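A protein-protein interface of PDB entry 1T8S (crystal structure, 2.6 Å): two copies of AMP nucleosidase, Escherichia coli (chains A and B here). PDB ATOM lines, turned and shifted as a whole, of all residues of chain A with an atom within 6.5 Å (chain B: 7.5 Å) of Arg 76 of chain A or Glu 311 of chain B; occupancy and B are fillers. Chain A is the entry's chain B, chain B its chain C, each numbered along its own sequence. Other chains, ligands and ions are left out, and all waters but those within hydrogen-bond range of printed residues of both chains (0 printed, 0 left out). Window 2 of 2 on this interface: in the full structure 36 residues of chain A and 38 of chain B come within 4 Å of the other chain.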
ATOM      1  N   PRO A  69      29.692 -12.224  13.916  1.00  0.00           N
ATOM      2  CA  PRO A  69      29.271 -13.082  15.032  1.00  0.00           C
ATOM      3  C   PRO A  69      28.647 -12.229  16.143  1.00  0.00           C
ATOM      4  O   PRO A  69      29.355 -11.628  16.952  1.00  0.00           O
ATOM      5  CB  PRO A  69      30.578 -13.740  15.471  1.00  0.00           C
ATOM      6  CG  PRO A  69      31.394 -13.758  14.205  1.00  0.00           C
ATOM      7  CD  PRO A  69      31.131 -12.389  13.642  1.00  0.00           C
ATOM      8  N   LYS A  70      27.321 -12.179  16.174  1.00  0.00           N
ATOM      9  CA  LYS A  70      26.615 -11.379  17.167  1.00  0.00           C
ATOM     10  C   LYS A  70      26.446 -12.105  18.499  1.00  0.00           C
ATOM     11  O   LYS A  70      26.190 -11.472  19.526  1.00  0.00           O
ATOM     12  CB  LYS A  70      25.230 -10.985  16.637  1.00  0.00           C
ATOM     13  CG  LYS A  70      25.224 -10.390  15.230  1.00  0.00           C
ATOM     14  CD  LYS A  70      25.877  -9.016  15.178  1.00  0.00           C
ATOM     15  CE  LYS A  70      25.065  -7.980  15.942  1.00  0.00           C
ATOM     16  NZ  LYS A  70      25.707  -6.632  15.892  1.00  0.00           N
ATOM     17  N   THR A  71      26.592 -13.428  18.485  1.00  0.00           N
ATOM     18  CA  THR A  71      26.413 -14.220  19.700  1.00  0.00           C
ATOM     19  C   THR A  71      27.689 -14.759  20.351  1.00  0.00           C
ATOM     20  O   THR A  71      27.664 -15.160  21.515  1.00  0.00           O
ATOM     21  CB  THR A  71      25.457 -15.408  19.438  1.00  0.00           C
ATOM     22  OG1 THR A  71      25.992 -16.238  18.401  1.00  0.00           O
ATOM     23  CG2 THR A  71      24.088 -14.903  19.010  1.00  0.00           C
ATOM     24  N   ARG A  72      28.796 -14.772  19.614  1.00  0.00           N
ATOM     25  CA  ARG A  72      30.056 -15.275  20.158  1.00  0.00           C
ATOM     26  C   ARG A  72      30.476 -14.460  21.380  1.00  0.00           C
ATOM     27  O   ARG A  72      30.271 -13.250  21.432  1.00  0.00           O
ATOM     28  CB  ARG A  72      31.145 -15.226  19.084  1.00  0.00           C
ATOM     29  CG  ARG A  72      32.442 -15.914  19.474  1.00  0.00           C
ATOM     30  CD  ARG A  72      33.317 -16.154  18.251  1.00  0.00           C
ATOM     31  NE  ARG A  72      33.600 -14.917  17.531  1.00  0.00           N
ATOM     32  CZ  ARG A  72      34.192 -14.862  16.343  1.00  0.00           C
ATOM     33  NH1 ARG A  72      34.566 -15.978  15.733  1.00  0.00           N
ATOM     34  NH2 ARG A  72      34.407 -13.690  15.759  1.00  0.00           N
ATOM     35  N   ALA A  73      31.065 -15.130  22.364  1.00  0.00           N
ATOM     36  CA  ALA A  73      31.489 -14.470  23.595  1.00  0.00           C
ATOM     37  C   ALA A  73      32.756 -13.624  23.456  1.00  0.00           C
ATOM     38  O   ALA A  73      32.920 -12.620  24.153  1.00  0.00           O
ATOM     39  CB  ALA A  73      31.682 -15.511  24.689  1.00  0.00           C
ATOM     40  N   PHE A  74      33.650 -14.026  22.560  1.00  0.00           N
ATOM     41  CA  PHE A  74      34.906 -13.308  22.365  1.00  0.00           C
ATOM     42  C   PHE A  74      35.249 -13.111  20.890  1.00  0.00           C
ATOM     43  O   PHE A  74      34.493 -13.516  20.006  1.00  0.00           O
ATOM     44  CB  PHE A  74      36.035 -14.065  23.077  1.00  0.00           C
ATOM     45  CG  PHE A  74      36.146 -15.514  22.670  1.00  0.00           C
ATOM     46  CD1 PHE A  74      36.801 -15.879  21.493  1.00  0.00           C
ATOM     47  CD2 PHE A  74      35.568 -16.515  23.451  1.00  0.00           C
ATOM     48  CE1 PHE A  74      36.878 -17.217  21.098  1.00  0.00           C
ATOM     49  CE2 PHE A  74      35.639 -17.855  23.065  1.00  0.00           C
ATOM     50  CZ  PHE A  74      36.296 -18.205  21.885  1.00  0.00           C
ATOM     51  N   GLY A  75      36.394 -12.486  20.631  1.00  0.00           N
ATOM     52  CA  GLY A  75      36.818 -12.248  19.265  1.00  0.00           C
ATOM     53  C   GLY A  75      35.812 -11.422  18.484  1.00  0.00           C
ATOM     54  O   GLY A  75      35.541 -11.703  17.317  1.00  0.00           O
ATOM     55  N   ARG A  76      35.257 -10.398  19.124  1.00  0.00           N
ATOM     56  CA  ARG A  76      34.277  -9.535  18.477  1.00  0.00           C
ATOM     57  C   ARG A  76      34.677  -8.073  18.528  1.00  0.00           C
ATOM     58  O   ARG A  76      35.523  -7.676  19.325  1.00  0.00           O
ATOM     59  CB  ARG A  76      32.913  -9.679  19.148  1.00  0.00           C
ATOM     60  CG  ARG A  76      32.162 -10.956  18.840  1.00  0.00           C
ATOM     61  CD  ARG A  76      30.862 -10.980  19.628  1.00  0.00           C
ATOM     62  NE  ARG A  76      30.082  -9.760  19.430  1.00  0.00           N
ATOM     63  CZ  ARG A  76      29.044  -9.394  20.182  1.00  0.00           C
ATOM     64  NH1 ARG A  76      28.643 -10.152  21.198  1.00  0.00           N
ATOM     65  NH2 ARG A  76      28.402  -8.262  19.919  1.00  0.00           N
ATOM     66  N   PHE A  77      34.054  -7.279  17.665  1.00  0.00           N
ATOM     67  CA  PHE A  77      34.295  -5.840  17.606  1.00  0.00           C
ATOM     68  C   PHE A  77      32.994  -5.140  17.967  1.00  0.00           C
ATOM     69  O   PHE A  77      31.941  -5.457  17.417  1.00  0.00           O
ATOM     70  CB  PHE A  77      34.724  -5.413  16.203  1.00  0.00           C
ATOM     71  CG  PHE A  77      36.159  -5.727  15.879  1.00  0.00           C
ATOM     72  CD1 PHE A  77      37.194  -5.090  16.558  1.00  0.00           C
ATOM     73  CD2 PHE A  77      36.475  -6.645  14.882  1.00  0.00           C
ATOM     74  CE1 PHE A  77      38.523  -5.361  16.246  1.00  0.00           C
ATOM     75  CE2 PHE A  77      37.800  -6.925  14.562  1.00  0.00           C
ATOM     76  CZ  PHE A  77      38.828  -6.280  15.245  1.00  0.00           C
ATOM     77  N   THR A  78      33.072  -4.197  18.900  1.00  0.00           N
ATOM     78  CA  THR A  78      31.897  -3.449  19.340  1.00  0.00           C
ATOM     79  C   THR A  78      31.697  -2.243  18.442  1.00  0.00           C
ATOM     80  O   THR A  78      30.591  -1.715  18.325  1.00  0.00           O
ATOM     81  CB  THR A  78      32.058  -2.950  20.803  1.00  0.00           C
ATOM     82  OG1 THR A  78      32.019  -4.069  21.700  1.00  0.00           O
ATOM     83  CG2 THR A  78      30.946  -1.961  21.171  1.00  0.00           C
ATOM     84  N   HIS A  79      32.777  -1.816  17.800  1.00  0.00           N
ATOM     85  CA  HIS A  79      32.734  -0.658  16.921  1.00  0.00           C
ATOM     86  C   HIS A  79      33.947  -0.653  16.000  1.00  0.00           C
ATOM     87  O   HIS A  79      34.874  -1.451  16.168  1.00  0.00           O
ATOM     88  CB  HIS A  79      32.715   0.618  17.765  1.00  0.00           C
ATOM     89  CG  HIS A  79      33.899   0.754  18.672  1.00  0.00           C
ATOM     90  ND1 HIS A  79      35.145   1.133  18.219  1.00  0.00           N
ATOM     91  CD2 HIS A  79      34.034   0.531  20.000  1.00  0.00           C
ATOM     92  CE1 HIS A  79      35.995   1.142  19.230  1.00  0.00           C
ATOM     93  NE2 HIS A  79      35.346   0.780  20.322  1.00  0.00           N
ATOM     94  N   TYR A  83      42.615  -1.165  17.331  1.00  0.00           N
ATOM     95  CA  TYR A  83      42.835  -1.761  18.642  1.00  0.00           C
ATOM     96  C   TYR A  83      44.294  -2.189  18.689  1.00  0.00           C
ATOM     97  O   TYR A  83      44.762  -2.904  17.804  1.00  0.00           O
ATOM     98  CB  TYR A  83      41.922  -2.968  18.843  1.00  0.00           C
ATOM     99  CG  TYR A  83      40.456  -2.639  18.713  1.00  0.00           C
ATOM    100  CD1 TYR A  83      39.878  -2.421  17.461  1.00  0.00           C
ATOM    101  CD2 TYR A  83      39.645  -2.528  19.842  1.00  0.00           C
ATOM    102  CE1 TYR A  83      38.524  -2.100  17.336  1.00  0.00           C
ATOM    103  CE2 TYR A  83      38.291  -2.208  19.731  1.00  0.00           C
ATOM    104  CZ  TYR A  83      37.737  -1.997  18.475  1.00  0.00           C
ATOM    105  OH  TYR A  83      36.399  -1.690  18.363  1.00  0.00           O
ATOM    106  N   LEU A 104      39.563 -12.546  14.065  1.00  0.00           N
ATOM    107  CA  LEU A 104      39.344 -11.181  13.601  1.00  0.00           C
ATOM    108  C   LEU A 104      39.658 -11.034  12.116  1.00  0.00           C
ATOM    109  O   LEU A 104      39.055 -10.216  11.421  1.00  0.00           O
ATOM    110  CB  LEU A 104      40.212 -10.205  14.401  1.00  0.00           C
ATOM    111  CG  LEU A 104      40.080 -10.229  15.926  1.00  0.00           C
ATOM    112  CD1 LEU A 104      41.009  -9.185  16.518  1.00  0.00           C
ATOM    113  CD2 LEU A 104      38.633  -9.968  16.339  1.00  0.00           C
ATOM    114  N   TYR A 108      35.991 -10.701  10.218  1.00  0.00           N
ATOM    115  CA  TYR A 108      35.778  -9.274  10.001  1.00  0.00           C
ATOM    116  C   TYR A 108      36.697  -8.723   8.915  1.00  0.00           C
ATOM    117  O   TYR A 108      36.526  -7.582   8.469  1.00  0.00           O
ATOM    118  CB  TYR A 108      36.018  -8.481  11.296  1.00  0.00           C
ATOM    119  CG  TYR A 108      35.011  -8.715  12.407  1.00  0.00           C
ATOM    120  CD1 TYR A 108      35.072  -9.854  13.214  1.00  0.00           C
ATOM    121  CD2 TYR A 108      34.007  -7.783  12.662  1.00  0.00           C
ATOM    122  CE1 TYR A 108      34.153 -10.052  14.253  1.00  0.00           C
ATOM    123  CE2 TYR A 108      33.086  -7.971  13.694  1.00  0.00           C
ATOM    124  CZ  TYR A 108      33.163  -9.101  14.486  1.00  0.00           C
ATOM    125  OH  TYR A 108      32.250  -9.261  15.507  1.00  0.00           O
ATOM    126  N   ARG A 473      28.655 -14.710  27.175  1.00  0.00           N
ATOM    127  CA  ARG A 473      28.773 -13.256  27.244  1.00  0.00           C
ATOM    128  C   ARG A 473      28.560 -12.695  28.645  1.00  0.00           C
ATOM    129  O   ARG A 473      28.679 -11.490  28.857  1.00  0.00           O
ATOM    130  CB  ARG A 473      27.772 -12.605  26.288  1.00  0.00           C
ATOM    131  CG  ARG A 473      28.039 -12.886  24.818  1.00  0.00           C
ATOM    132  CD  ARG A 473      26.860 -12.443  23.944  1.00  0.00           C
ATOM    133  NE  ARG A 473      25.640 -13.203  24.234  1.00  0.00           N
ATOM    134  CZ  ARG A 473      24.495 -13.068  23.564  1.00  0.00           C
ATOM    135  NH1 ARG A 473      24.413 -12.200  22.564  1.00  0.00           N
ATOM    136  NH2 ARG A 473      23.434 -13.802  23.888  1.00  0.00           N
ATOM    137  N   ARG A 476      31.445 -10.451  29.620  1.00  0.00           N
ATOM    138  CA  ARG A 476      31.827  -9.359  28.719  1.00  0.00           C
ATOM    139  C   ARG A 476      31.522  -7.971  29.262  1.00  0.00           C
ATOM    140  O   ARG A 476      30.436  -7.711  29.781  1.00  0.00           O
ATOM    141  CB  ARG A 476      31.110  -9.474  27.373  1.00  0.00           C
ATOM    142  CG  ARG A 476      31.611 -10.557  26.443  1.00  0.00           C
ATOM    143  CD  ARG A 476      30.799 -10.505  25.146  1.00  0.00           C
ATOM    144  NE  ARG A 476      30.946  -9.220  24.457  1.00  0.00           N
ATOM    145  CZ  ARG A 476      32.027  -8.866  23.758  1.00  0.00           C
ATOM    146  NH1 ARG A 476      33.062  -9.705  23.651  1.00  0.00           N
ATOM    147  NH2 ARG A 476      32.074  -7.677  23.159  1.00  0.00           N
ATOM    148  N   GLU A 480      34.871  -4.391  26.125  1.00  0.00           N
ATOM    149  CA  GLU A 480      35.590  -5.661  26.058  1.00  0.00           C
ATOM    150  C   GLU A 480      36.641  -5.697  24.951  1.00  0.00           C
ATOM    151  O   GLU A 480      36.349  -5.371  23.795  1.00  0.00           O
ATOM    152  CB  GLU A 480      34.593  -6.810  25.851  1.00  0.00           C
ATOM    153  CG  GLU A 480      35.153  -8.208  26.088  1.00  0.00           C
ATOM    154  CD  GLU A 480      35.606  -8.449  27.531  1.00  0.00           C
ATOM    155  OE1 GLU A 480      34.947  -7.948  28.475  1.00  0.00           O
ATOM    156  OE2 GLU A 480      36.620  -9.164  27.721  1.00  0.00           O
ATOM    157  N   PRO A 481      37.886  -6.067  25.300  1.00  0.00           N
ATOM    158  CA  PRO A 481      38.965  -6.151  24.308  1.00  0.00           C
ATOM    159  C   PRO A 481      38.607  -7.301  23.355  1.00  0.00           C
ATOM    160  O   PRO A 481      37.952  -8.274  23.761  1.00  0.00           O
ATOM    161  CB  PRO A 481      40.191  -6.489  25.154  1.00  0.00           C
ATOM    162  CG  PRO A 481      39.868  -5.893  26.502  1.00  0.00           C
ATOM    163  CD  PRO A 481      38.407  -6.232  26.669  1.00  0.00           C
ATOM    164  N   PRO A 482      39.009  -7.200  22.076  1.00  0.00           N
ATOM    165  CA  PRO A 482      38.724  -8.239  21.079  1.00  0.00           C
ATOM    166  C   PRO A 482      39.266  -9.625  21.472  1.00  0.00           C
ATOM    167  O   PRO A 482      38.570 -10.639  21.317  1.00  0.00           O
ATOM    168  CB  PRO A 482      39.381  -7.683  19.824  1.00  0.00           C
ATOM    169  CG  PRO A 482      39.179  -6.204  19.993  1.00  0.00           C
ATOM    170  CD  PRO A 482      39.579  -6.002  21.433  1.00  0.00           C
ATOM    171  N   PHE A 483      40.498  -9.660  21.983  1.00  0.00           N
ATOM    172  CA  PHE A 483      41.130 -10.911  22.413  1.00  0.00           C
ATOM    173  C   PHE A 483      40.422 -11.555  23.614  1.00  0.00           C
ATOM    174  O   PHE A 483      40.092 -10.872  24.592  1.00  0.00           O
ATOM    175  CB  PHE A 483      42.599 -10.656  22.773  1.00  0.00           C
ATOM    176  CG  PHE A 483      43.503 -10.517  21.582  1.00  0.00           C
ATOM    177  CD1 PHE A 483      42.974 -10.369  20.296  1.00  0.00           C
ATOM    178  CD2 PHE A 483      44.887 -10.558  21.739  1.00  0.00           C
ATOM    179  CE1 PHE A 483      43.816 -10.270  19.185  1.00  0.00           C
ATOM    180  CE2 PHE A 483      45.740 -10.459  20.634  1.00  0.00           C
ATOM    181  CZ  PHE A 483      45.203 -10.316  19.357  1.00  0.00           C
ATOM    182  N   GLY B 308      17.325  -1.632  26.737  1.00  0.00           N
ATOM    183  CA  GLY B 308      18.454  -2.478  26.387  1.00  0.00           C
ATOM    184  C   GLY B 308      19.705  -1.630  26.442  1.00  0.00           C
ATOM    185  O   GLY B 308      19.706  -0.515  25.943  1.00  0.00           O
ATOM    186  N   LEU B 309      20.771  -2.136  27.046  1.00  0.00           N
ATOM    187  CA  LEU B 309      21.995  -1.358  27.153  1.00  0.00           C
ATOM    188  C   LEU B 309      23.109  -1.751  26.176  1.00  0.00           C
ATOM    189  O   LEU B 309      24.131  -1.074  26.090  1.00  0.00           O
ATOM    190  CB  LEU B 309      22.523  -1.447  28.582  1.00  0.00           C
ATOM    191  CG  LEU B 309      21.590  -0.961  29.690  1.00  0.00           C
ATOM    192  CD1 LEU B 309      22.176  -1.294  31.076  1.00  0.00           C
ATOM    193  CD2 LEU B 309      21.379   0.531  29.524  1.00  0.00           C
ATOM    194  N   ARG B 310      22.921  -2.839  25.437  1.00  0.00           N
ATOM    195  CA  ARG B 310      23.943  -3.299  24.497  1.00  0.00           C
ATOM    196  C   ARG B 310      23.635  -2.933  23.054  1.00  0.00           C
ATOM    197  O   ARG B 310      22.495  -3.026  22.612  1.00  0.00           O
ATOM    198  CB  ARG B 310      24.112  -4.814  24.608  1.00  0.00           C
ATOM    199  CG  ARG B 310      24.563  -5.281  25.978  1.00  0.00           C
ATOM    200  CD  ARG B 310      25.824  -4.558  26.413  1.00  0.00           C
ATOM    201  NE  ARG B 310      26.233  -4.967  27.745  1.00  0.00           N
ATOM    202  CZ  ARG B 310      27.150  -5.890  27.997  1.00  0.00           C
ATOM    203  NH1 ARG B 310      27.767  -6.507  26.999  1.00  0.00           N
ATOM    204  NH2 ARG B 310      27.448  -6.190  29.252  1.00  0.00           N
ATOM    205  N   GLU B 311      24.658  -2.533  22.309  1.00  0.00           N
ATOM    206  CA  GLU B 311      24.456  -2.152  20.917  1.00  0.00           C
ATOM    207  C   GLU B 311      23.875  -3.282  20.072  1.00  0.00           C
ATOM    208  O   GLU B 311      23.065  -3.031  19.181  1.00  0.00           O
ATOM    209  CB  GLU B 311      25.776  -1.667  20.313  1.00  0.00           C
ATOM    210  CG  GLU B 311      26.869  -2.731  20.259  1.00  0.00           C
ATOM    211  CD  GLU B 311      26.894  -3.491  18.932  1.00  0.00           C
ATOM    212  OE1 GLU B 311      27.631  -4.508  18.847  1.00  0.00           O
ATOM    213  OE2 GLU B 311      26.185  -3.066  17.982  1.00  0.00           O
ATOM    214  N   SER B 312      24.271  -4.521  20.360  1.00  0.00           N
ATOM    215  CA  SER B 312      23.784  -5.670  19.597  1.00  0.00           C
ATOM    216  C   SER B 312      22.328  -6.037  19.899  1.00  0.00           C
ATOM    217  O   SER B 312      21.763  -6.919  19.259  1.00  0.00           O
ATOM    218  CB  SER B 312      24.670  -6.892  19.847  1.00  0.00           C
ATOM    219  OG  SER B 312      24.503  -7.373  21.169  1.00  0.00           O
ATOM    220  N   GLN B 313      21.722  -5.380  20.880  1.00  0.00           N
ATOM    221  CA  GLN B 313      20.335  -5.660  21.219  1.00  0.00           C
ATOM    222  C   GLN B 313      19.402  -4.908  20.293  1.00  0.00           C
ATOM    223  O   GLN B 313      19.686  -3.790  19.874  1.00  0.00           O
ATOM    224  CB  GLN B 313      20.030  -5.251  22.654  1.00  0.00           C
ATOM    225  CG  GLN B 313      20.148  -6.365  23.668  1.00  0.00           C
ATOM    226  CD  GLN B 313      20.151  -5.845  25.087  1.00  0.00           C
ATOM    227  OE1 GLN B 313      19.881  -6.590  26.032  1.00  0.00           O
ATOM    228  NE2 GLN B 313      20.467  -4.562  25.251  1.00  0.00           N
ATOM    229  N   ALA B 314      18.274  -5.525  19.982  1.00  0.00           N
ATOM    230  CA  ALA B 314      17.300  -4.911  19.106  1.00  0.00           C
ATOM    231  C   ALA B 314      15.986  -4.800  19.842  1.00  0.00           C
ATOM    232  O   ALA B 314      15.628  -5.669  20.635  1.00  0.00           O
ATOM    233  CB  ALA B 314      17.120  -5.751  17.861  1.00  0.00           C
ATOM    234  N   ARG B 371      19.000 -12.675  25.440  1.00  0.00           N
ATOM    235  CA  ARG B 371      20.262 -12.409  26.113  1.00  0.00           C
ATOM    236  C   ARG B 371      20.032 -12.689  27.605  1.00  0.00           C
ATOM    237  O   ARG B 371      19.018 -12.273  28.183  1.00  0.00           O
ATOM    238  CB  ARG B 371      20.672 -10.946  25.870  1.00  0.00           C
ATOM    239  CG  ARG B 371      21.923 -10.442  26.592  1.00  0.00           C
ATOM    240  CD  ARG B 371      23.197 -11.166  26.145  1.00  0.00           C
ATOM    241  NE  ARG B 371      24.433 -10.450  26.505  1.00  0.00           N
ATOM    242  CZ  ARG B 371      24.937  -9.429  25.813  1.00  0.00           C
ATOM    243  NH1 ARG B 371      24.319  -8.991  24.720  1.00  0.00           N
ATOM    244  NH2 ARG B 371      26.068  -8.853  26.200  1.00  0.00           N
ATOM    245  N   LYS B 429      16.367   1.722  23.431  1.00  0.00           N
ATOM    246  CA  LYS B 429      17.808   1.639  23.571  1.00  0.00           C
ATOM    247  C   LYS B 429      18.337   3.024  23.876  1.00  0.00           C
ATOM    248  O   LYS B 429      18.824   3.726  22.997  1.00  0.00           O
ATOM    249  CB  LYS B 429      18.429   1.081  22.303  1.00  0.00           C
ATOM    250  CG  LYS B 429      17.970  -0.332  22.013  1.00  0.00           C
ATOM    251  CD  LYS B 429      18.694  -0.908  20.814  1.00  0.00           C
ATOM    252  CE  LYS B 429      20.159  -1.096  21.131  1.00  0.00           C
ATOM    253  NZ  LYS B 429      20.204  -1.808  22.425  1.00  0.00           N
ATOM    254  N   LEU B 431      21.006   4.216  25.312  1.00  0.00           N
ATOM    255  CA  LEU B 431      22.382   4.513  24.979  1.00  0.00           C
ATOM    256  C   LEU B 431      22.673   4.580  23.481  1.00  0.00           C
ATOM    257  O   LEU B 431      23.727   5.066  23.082  1.00  0.00           O
ATOM    258  CB  LEU B 431      23.290   3.470  25.630  1.00  0.00           C
ATOM    259  CG  LEU B 431      23.802   3.699  27.061  1.00  0.00           C
ATOM    260  CD1 LEU B 431      22.818   4.490  27.898  1.00  0.00           C
ATOM    261  CD2 LEU B 431      24.086   2.358  27.678  1.00  0.00           C
ATOM    262  N   HIS B 432      21.746   4.121  22.648  1.00  0.00           N
ATOM    263  CA  HIS B 432      22.002   4.127  21.210  1.00  0.00           C
ATOM    264  C   HIS B 432      20.977   4.834  20.322  1.00  0.00           C
ATOM    265  O   HIS B 432      20.640   4.344  19.246  1.00  0.00           O
ATOM    266  CB  HIS B 432      22.190   2.687  20.708  1.00  0.00           C
ATOM    267  CG  HIS B 432      23.197   1.903  21.490  1.00  0.00           C
ATOM    268  ND1 HIS B 432      22.873   1.218  22.640  1.00  0.00           N
ATOM    269  CD2 HIS B 432      24.528   1.733  21.315  1.00  0.00           C
ATOM    270  CE1 HIS B 432      23.960   0.661  23.141  1.00  0.00           C
ATOM    271  NE2 HIS B 432      24.980   0.960  22.356  1.00  0.00           N
ATOM    272  N   GLU B 434      17.513   5.389  20.023  1.00  0.00           N
ATOM    273  CA  GLU B 434      16.356   4.601  19.574  1.00  0.00           C
ATOM    274  C   GLU B 434      15.445   4.612  20.802  1.00  0.00           C
ATOM    275  O   GLU B 434      14.802   3.617  21.138  1.00  0.00           O
ATOM    276  CB  GLU B 434      16.743   3.159  19.225  1.00  0.00           C
ATOM    277  CG  GLU B 434      17.589   2.996  17.966  1.00  0.00           C
ATOM    278  CD  GLU B 434      17.845   1.530  17.611  1.00  0.00           C
ATOM    279  OE1 GLU B 434      16.861   0.814  17.309  1.00  0.00           O
ATOM    280  OE2 GLU B 434      19.025   1.094  17.637  1.00  0.00           O
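The backbone carbonyl oxygen (O) of Arg 476 of chain A is in hydrogen-bond range of the guanidinium group (NH2) of Arg 310 of chain B, 3.4 Å away. The guanidinium group (NH2) of Arg 76 of chain A is in salt-bridge range of the side-chain carboxylate (OE1) of Glu 311 of chain B, 3.98 Å away.
O of Pro 69 of chain A lies close to NE of Arg 76 of chain A (3.2 Å). The side-chain amide nitrogen (NE2) of Gln 313 of chain B sits close to the backbone NH (N) of Arg 310 of chain B (3.0 Å). The guanidinium group of Arg 476 of chain A is in hydrogen-bond range of the backbone carbonyl oxygen of Ala 73 of chain A. The guanidinium group (NH1) of Arg 76 of chain A is in hydrogen-bond range of the backbone carbonyl oxygen (O) of Lys 70 of chain A, at 3.2 Å. The backbone carbonyl oxygen (O) of Arg 310 of chain B lies within hydrogen-bond range of the side-chain amino group (NZ) of Lys 429 of chain B, 2.6 Å away.
Among the printed residues, merely in contact across the chains: Arg 76 of chain A with Ser 312 of chain B and Arg 473 of chain A with Arg 371 of chain B.
Of chain B, only Glu 311 and Ser 312 come within 4 Å of Arg 76 of chain A. Of chain A, only Arg 76 comes within 4 Å of Glu 311 of chain B. No residue of chain B comes within 4 Å of Gly 75 of chain A. Printed residues of chain A within 4 Å of Arg 310 of chain B: Arg 476. Of the printed residues of chain B, Arg 473 of chain A touches Arg 371 (3.5 Å). Of the printed residues of chain B, Arg 476 of chain A touches Arg 310. Ala 73 of chain A touches none of the printed residues of chain B. Phe 77 of chain A touches none of the printed residues of chain B. The nearest printed residue of chain A that does not touch Glu 311 of chain B is Thr 78 of chain A (4.1 Å).
Of the 20 printed residues of chain A, 3 touch a printed residue of chain B. Printed residues of chain A that touch a printed residue of chain B: Arg 76, Arg 473 and Arg 476. Printed residues of chain B that touch a printed residue of chain A: Arg 310, Glu 311, Ser 312 and Arg 371.
No position is printed for both chains. Of the 4 pairs that touch across the chains among the printed residues, none has its exchanged pair printed and touching as well.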
